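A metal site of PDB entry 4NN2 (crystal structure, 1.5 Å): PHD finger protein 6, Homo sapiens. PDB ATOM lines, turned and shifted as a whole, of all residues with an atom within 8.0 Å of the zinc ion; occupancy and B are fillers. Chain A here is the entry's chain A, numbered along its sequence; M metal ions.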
ATOM      1  N   LYS A   7      12.623  -3.791  19.202  1.00  0.00           N
ATOM      2  CA  LYS A   7      11.919  -4.053  20.452  1.00  0.00           C
ATOM      3  C   LYS A   7      12.196  -5.467  20.917  1.00  0.00           C
ATOM      4  O   LYS A   7      12.501  -6.365  20.138  1.00  0.00           O
ATOM      5  CB  LYS A   7      10.410  -3.797  20.310  1.00  0.00           C
ATOM      6  CG  LYS A   7       9.703  -4.601  19.251  1.00  0.00           C
ATOM      7  CD  LYS A   7       8.257  -4.118  19.074  1.00  0.00           C
ATOM      8  CE  LYS A   7       7.509  -4.876  17.996  1.00  0.00           C
ATOM      9  NZ  LYS A   7       8.196  -4.832  16.675  1.00  0.00           N
ATOM     10  N   CYS A   8      12.098  -5.648  22.231  1.00  0.00           N
ATOM     11  CA  CYS A   8      12.311  -6.941  22.850  1.00  0.00           C
ATOM     12  C   CYS A   8      11.354  -7.995  22.306  1.00  0.00           C
ATOM     13  O   CYS A   8      10.151  -7.758  22.207  1.00  0.00           O
ATOM     14  CB  CYS A   8      12.132  -6.762  24.356  1.00  0.00           C
ATOM     15  SG  CYS A   8      12.332  -8.276  25.333  1.00  0.00           S
ATOM     16  N   GLY A   9      11.887  -9.156  21.966  1.00  0.00           N
ATOM     17  CA  GLY A   9      11.096 -10.249  21.400  1.00  0.00           C
ATOM     18  C   GLY A   9      10.172 -10.893  22.410  1.00  0.00           C
ATOM     19  O   GLY A   9       9.282 -11.647  22.031  1.00  0.00           O
ATOM     20  N   PHE A  10      10.413 -10.614  23.686  1.00  0.00           N
ATOM     21  CA  PHE A  10       9.581 -11.132  24.760  1.00  0.00           C
ATOM     22  C   PHE A  10       8.457 -10.174  25.153  1.00  0.00           C
ATOM     23  O   PHE A  10       7.266 -10.535  25.096  1.00  0.00           O
ATOM     24  CB  PHE A  10      10.468 -11.465  25.977  1.00  0.00           C
ATOM     25  CG  PHE A  10      11.505 -12.517  25.691  1.00  0.00           C
ATOM     26  CD1 PHE A  10      11.130 -13.826  25.454  1.00  0.00           C
ATOM     27  CD2 PHE A  10      12.852 -12.187  25.619  1.00  0.00           C
ATOM     28  CE1 PHE A  10      12.076 -14.804  25.178  1.00  0.00           C
ATOM     29  CE2 PHE A  10      13.801 -13.156  25.338  1.00  0.00           C
ATOM     30  CZ  PHE A  10      13.419 -14.470  25.129  1.00  0.00           C
ATOM     31  N   CYS A  11       8.815  -8.958  25.564  1.00  0.00           N
ATOM     32  CA  CYS A  11       7.849  -8.008  26.101  1.00  0.00           C
ATOM     33  C   CYS A  11       7.403  -6.929  25.101  1.00  0.00           C
ATOM     34  O   CYS A  11       6.501  -6.153  25.415  1.00  0.00           O
ATOM     35  CB  CYS A  11       8.358  -7.346  27.384  1.00  0.00           C
ATOM     36  SG  CYS A  11       9.690  -6.151  27.121  1.00  0.00           S
ATOM     37  N   HIS A  12       8.023  -6.888  23.927  1.00  0.00           N
ATOM     38  CA  HIS A  12       7.554  -6.044  22.806  1.00  0.00           C
ATOM     39  C   HIS A  12       7.790  -4.558  23.007  1.00  0.00           C
ATOM     40  O   HIS A  12       7.134  -3.738  22.366  1.00  0.00           O
ATOM     41  CB  HIS A  12       6.067  -6.310  22.519  1.00  0.00           C
ATOM     42  CG  HIS A  12       5.728  -7.753  22.527  1.00  0.00           C
ATOM     43  ND1 HIS A  12       6.272  -8.642  21.637  1.00  0.00           N
ATOM     44  CD2 HIS A  12       4.956  -8.477  23.362  1.00  0.00           C
ATOM     45  CE1 HIS A  12       5.831  -9.858  21.903  1.00  0.00           C
ATOM     46  NE2 HIS A  12       5.021  -9.780  22.947  1.00  0.00           N
ATOM     47  N   VAL A  13       8.745  -4.215  23.871  1.00  0.00           N
ATOM     48  CA  VAL A  13       9.136  -2.815  24.126  1.00  0.00           C
ATOM     49  C   VAL A  13      10.623  -2.639  23.852  1.00  0.00           C
ATOM     50  O   VAL A  13      11.421  -3.563  24.060  1.00  0.00           O
ATOM     51  CB  VAL A  13       8.787  -2.396  25.552  1.00  0.00           C
ATOM     52  CG1 VAL A  13       9.142  -0.920  25.819  1.00  0.00           C
ATOM     53  CG2 VAL A  13       7.298  -2.628  25.809  1.00  0.00           C
ATOM     54  N   GLY A  14      10.998  -1.452  23.376  1.00  0.00           N
ATOM     55  CA  GLY A  14      12.393  -1.121  23.069  1.00  0.00           C
ATOM     56  C   GLY A  14      13.180  -0.520  24.237  1.00  0.00           C
ATOM     57  O   GLY A  14      12.912  -0.793  25.415  1.00  0.00           O
ATOM     58  N   GLU A  17      12.501   1.059  28.118  1.00  0.00           N
ATOM     59  CA  GLU A  17      12.418   0.322  29.367  1.00  0.00           C
ATOM     60  C   GLU A  17      13.739  -0.321  29.784  1.00  0.00           C
ATOM     61  O   GLU A  17      13.743  -1.228  30.608  1.00  0.00           O
ATOM     62  CB  GLU A  17      11.320  -0.739  29.289  1.00  0.00           C
ATOM     63  CG  GLU A  17       9.908  -0.177  29.296  1.00  0.00           C
ATOM     64  CD  GLU A  17       9.504   0.459  30.607  1.00  0.00           C
ATOM     65  OE1 GLU A  17      10.169   0.268  31.659  1.00  0.00           O
ATOM     66  OE2 GLU A  17       8.471   1.173  30.612  1.00  0.00           O
ATOM     67  N   ARG A  21      13.960  -3.064  32.867  1.00  0.00           N
ATOM     68  CA  ARG A  21      13.968  -4.420  32.323  1.00  0.00           C
ATOM     69  C   ARG A  21      15.366  -4.891  31.892  1.00  0.00           C
ATOM     70  O   ARG A  21      15.526  -6.042  31.468  1.00  0.00           O
ATOM     71  CB  ARG A  21      12.974  -4.515  31.167  1.00  0.00           C
ATOM     72  CG  ARG A  21      11.569  -4.081  31.572  1.00  0.00           C
ATOM     73  CD  ARG A  21      10.529  -4.188  30.476  1.00  0.00           C
ATOM     74  NE  ARG A  21       9.284  -3.524  30.890  1.00  0.00           N
ATOM     75  CZ  ARG A  21       8.174  -3.451  30.182  1.00  0.00           C
ATOM     76  NH1 ARG A  21       8.076  -4.013  28.984  1.00  0.00           N
ATOM     77  NH2 ARG A  21       7.118  -2.792  30.679  1.00  0.00           N
ATOM     78  N   GLY A  22      16.361  -4.015  32.000  1.00  0.00           N
ATOM     79  CA  GLY A  22      17.712  -4.297  31.550  1.00  0.00           C
ATOM     80  C   GLY A  22      17.933  -3.862  30.128  1.00  0.00           C
ATOM     81  O   GLY A  22      16.988  -3.787  29.330  1.00  0.00           O
ATOM     82  N   LYS A  23      19.195  -3.608  29.783  1.00  0.00           N
ATOM     83  CA  LYS A  23      19.557  -3.108  28.462  1.00  0.00           C
ATOM     84  C   LYS A  23      19.034  -3.994  27.337  1.00  0.00           C
ATOM     85  O   LYS A  23      19.163  -5.217  27.392  1.00  0.00           O
ATOM     86  CB  LYS A  23      21.078  -2.984  28.332  1.00  0.00           C
ATOM     87  CG  LYS A  23      21.520  -2.335  27.034  1.00  0.00           C
ATOM     88  CD  LYS A  23      23.018  -2.082  26.989  1.00  0.00           C
ATOM     89  CE  LYS A  23      23.393  -1.353  25.700  1.00  0.00           C
ATOM     90  NZ  LYS A  23      22.636  -0.081  25.510  1.00  0.00           N
ATOM     91  N   LEU A  24      18.496  -3.361  26.293  1.00  0.00           N
ATOM     92  CA  LEU A  24      18.086  -4.069  25.091  1.00  0.00           C
ATOM     93  C   LEU A  24      19.312  -4.490  24.285  1.00  0.00           C
ATOM     94  O   LEU A  24      20.095  -3.629  23.876  1.00  0.00           O
ATOM     95  CB  LEU A  24      17.184  -3.190  24.219  1.00  0.00           C
ATOM     96  CG  LEU A  24      16.473  -3.920  23.064  1.00  0.00           C
ATOM     97  CD1 LEU A  24      15.343  -4.779  23.562  1.00  0.00           C
ATOM     98  CD2 LEU A  24      15.949  -2.913  22.072  1.00  0.00           C
ATOM     99  N   ALA A  33      15.784  -9.235  19.304  1.00  0.00           N
ATOM    100  CA  ALA A  33      16.327  -8.463  20.408  1.00  0.00           C
ATOM    101  C   ALA A  33      15.695  -8.899  21.731  1.00  0.00           C
ATOM    102  O   ALA A  33      14.639  -9.527  21.735  1.00  0.00           O
ATOM    103  CB  ALA A  33      16.065  -6.972  20.196  1.00  0.00           C
ATOM    104  N   ALA A  34      16.328  -8.540  22.834  1.00  0.00           N
ATOM    105  CA  ALA A  34      15.759  -8.808  24.165  1.00  0.00           C
ATOM    106  C   ALA A  34      16.407  -7.927  25.231  1.00  0.00           C
ATOM    107  O   ALA A  34      17.619  -7.691  25.189  1.00  0.00           O
ATOM    108  CB  ALA A  34      15.951 -10.257  24.539  1.00  0.00           C
ATOM    109  N   HIS A  35      15.610  -7.441  26.167  1.00  0.00           N
ATOM    110  CA  HIS A  35      16.138  -6.797  27.367  1.00  0.00           C
ATOM    111  C   HIS A  35      16.900  -7.843  28.167  1.00  0.00           C
ATOM    112  O   HIS A  35      16.538  -9.018  28.177  1.00  0.00           O
ATOM    113  CB  HIS A  35      15.044  -6.242  28.267  1.00  0.00           C
ATOM    114  CG  HIS A  35      14.227  -5.157  27.648  1.00  0.00           C
ATOM    115  ND1 HIS A  35      12.897  -5.331  27.335  1.00  0.00           N
ATOM    116  CD2 HIS A  35      14.523  -3.879  27.313  1.00  0.00           C
ATOM    117  CE1 HIS A  35      12.421  -4.221  26.807  1.00  0.00           C
ATOM    118  NE2 HIS A  35      13.382  -3.327  26.776  1.00  0.00           N
ATOM    119  N   TYR A  36      17.936  -7.390  28.870  1.00  0.00           N
ATOM    120  CA  TYR A  36      18.742  -8.264  29.694  1.00  0.00           C
ATOM    121  C   TYR A  36      17.907  -9.142  30.645  1.00  0.00           C
ATOM    122  O   TYR A  36      18.116 -10.349  30.697  1.00  0.00           O
ATOM    123  CB  TYR A  36      19.748  -7.425  30.472  1.00  0.00           C
ATOM    124  CG  TYR A  36      20.580  -8.204  31.463  1.00  0.00           C
ATOM    125  CD1 TYR A  36      21.426  -9.230  31.049  1.00  0.00           C
ATOM    126  CD2 TYR A  36      20.540  -7.909  32.819  1.00  0.00           C
ATOM    127  CE1 TYR A  36      22.205  -9.927  31.959  1.00  0.00           C
ATOM    128  CE2 TYR A  36      21.312  -8.607  33.744  1.00  0.00           C
ATOM    129  CZ  TYR A  36      22.147  -9.613  33.300  1.00  0.00           C
ATOM    130  OH  TYR A  36      22.938 -10.305  34.203  1.00  0.00           O
ATOM    131  N   LYS A  37      17.000  -8.557  31.407  1.00  0.00           N
ATOM    132  CA  LYS A  37      16.265  -9.381  32.387  1.00  0.00           C
ATOM    133  C   LYS A  37      15.261 -10.312  31.714  1.00  0.00           C
ATOM    134  O   LYS A  37      15.052 -11.443  32.167  1.00  0.00           O
ATOM    135  CB  LYS A  37      15.597  -8.516  33.446  1.00  0.00           C
ATOM    136  CG  LYS A  37      16.610  -7.701  34.246  1.00  0.00           C
ATOM    137  CD  LYS A  37      16.015  -7.113  35.503  1.00  0.00           C
ATOM    138  CE  LYS A  37      17.065  -6.405  36.356  1.00  0.00           C
ATOM    139  NZ  LYS A  37      16.462  -5.823  37.583  1.00  0.00           N
ATOM    140  N   CYS A  38      14.651  -9.849  30.619  1.00  0.00           N
ATOM    141  CA  CYS A  38      13.727 -10.690  29.869  1.00  0.00           C
ATOM    142  C   CYS A  38      14.415 -11.951  29.364  1.00  0.00           C
ATOM    143  O   CYS A  38      13.832 -13.046  29.421  1.00  0.00           O
ATOM    144  CB  CYS A  38      13.119  -9.882  28.714  1.00  0.00           C
ATOM    145  SG  CYS A  38      12.110  -8.473  29.246  1.00  0.00           S
ATOM    146  N   MET A  39      15.644 -11.825  28.871  1.00  0.00           N
ATOM    147  CA  MET A  39      16.386 -12.995  28.417  1.00  0.00           C
ATOM    148  C   MET A  39      16.990 -13.787  29.577  1.00  0.00           C
ATOM    149  O   MET A  39      16.983 -15.012  29.557  1.00  0.00           O
ATOM    150  CB  MET A  39      17.437 -12.635  27.361  1.00  0.00           C
ATOM    151  CG  MET A  39      18.539 -11.682  27.792  1.00  0.00           C
ATOM    152  SD  MET A  39      19.873 -11.616  26.573  1.00  0.00           S
ATOM    153  CE  MET A  39      20.785 -13.073  26.987  1.00  0.00           C
ATOM    154  N   GLY A  83       4.816 -13.935  24.506  1.00  0.00           N
ATOM    155  CA  GLY A  83       6.198 -13.613  24.865  1.00  0.00           C
ATOM    156  C   GLY A  83       6.550 -13.908  26.298  1.00  0.00           C
ATOM    157  O   GLY A  83       7.670 -13.629  26.724  1.00  0.00           O
ATOM    158  N   HIS A  98       5.972 -12.366  31.435  1.00  0.00           N
ATOM    159  CA  HIS A  98       6.957 -11.336  31.085  1.00  0.00           C
ATOM    160  C   HIS A  98       7.647 -10.867  32.372  1.00  0.00           C
ATOM    161  O   HIS A  98       7.030 -10.866  33.439  1.00  0.00           O
ATOM    162  CB  HIS A  98       6.286 -10.131  30.443  1.00  0.00           C
ATOM    163  CG  HIS A  98       5.551 -10.440  29.188  1.00  0.00           C
ATOM    164  ND1 HIS A  98       4.169 -10.420  29.117  1.00  0.00           N
ATOM    165  CD2 HIS A  98       5.991 -10.783  27.961  1.00  0.00           C
ATOM    166  CE1 HIS A  98       3.799 -10.718  27.878  1.00  0.00           C
ATOM    167  NE2 HIS A  98       4.885 -10.947  27.160  1.00  0.00           N
ATOM    168  N   TYR A  99       8.895 -10.435  32.274  1.00  0.00           N
ATOM    169  CA  TYR A  99       9.629 -10.031  33.469  1.00  0.00           C
ATOM    170  C   TYR A  99       8.859  -9.039  34.348  1.00  0.00           C
ATOM    171  O   TYR A  99       8.644  -9.291  35.541  1.00  0.00           O
ATOM    172  CB  TYR A  99      11.028  -9.478  33.118  1.00  0.00           C
ATOM    173  CG  TYR A  99      11.701  -8.887  34.324  1.00  0.00           C
ATOM    174  CD1 TYR A  99      12.225  -9.713  35.318  1.00  0.00           C
ATOM    175  CD2 TYR A  99      11.763  -7.514  34.509  1.00  0.00           C
ATOM    176  CE1 TYR A  99      12.809  -9.179  36.457  1.00  0.00           C
ATOM    177  CE2 TYR A  99      12.325  -6.978  35.644  1.00  0.00           C
ATOM    178  CZ  TYR A  99      12.852  -7.803  36.601  1.00  0.00           C
ATOM    179  OH  TYR A  99      13.427  -7.266  37.742  1.00  0.00           O
ATOM    180  N   HIS A 100       8.440  -7.923  33.771  1.00  0.00           N
ATOM    181  CA  HIS A 100       7.739  -6.895  34.556  1.00  0.00           C
ATOM    182  C   HIS A 100       6.393  -7.376  35.087  1.00  0.00           C
ATOM    183  O   HIS A 100       5.965  -6.977  36.173  1.00  0.00           O
ATOM    184  CB  HIS A 100       7.584  -5.584  33.773  1.00  0.00           C
ATOM    185  CG  HIS A 100       6.621  -5.663  32.633  1.00  0.00           C
ATOM    186  ND1 HIS A 100       6.884  -6.362  31.481  1.00  0.00           N
ATOM    187  CD2 HIS A 100       5.401  -5.095  32.465  1.00  0.00           C
ATOM    188  CE1 HIS A 100       5.853  -6.245  30.660  1.00  0.00           C
ATOM    189  NE2 HIS A 100       4.955  -5.457  31.230  1.00  0.00           N
HETATM  190 ZN    ZN M   1      11.746  -7.168  27.392  1.00  0.00          ZN
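ND1 of His 35 is bound to the zinc ion. The zinc ion is bound by SG of Cys 38 (2.3 Å). SG of Cys 11 is bound to the zinc ion (2.3 Å). The zinc ion is bound by the side-chain sulfur (SG) of Cys 8 (2.4 Å).
A ring nitrogen (NE2) of His 35 sits close to the backbone carbonyl oxygen of Val 13 (3.4 Å). A ring nitrogen (NE2) of His 35 lies within hydrogen-bond range of the backbone carbonyl oxygen (O) of Gly 14. The side-chain sulfur (SG) of Cys 11 sits close to the guanidinium group (NH1) of Arg 21, 3.3 Å away. SG of Cys 8 sits close to N of Phe 10 (3.4 Å). O of Val 13 lies within hydrogen-bond range of N of Cys 8 (2.9 Å).
Four residues have an atom within 4 Å of the zinc ion: Cys 8, Cys 11, His 35 and Cys 38.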
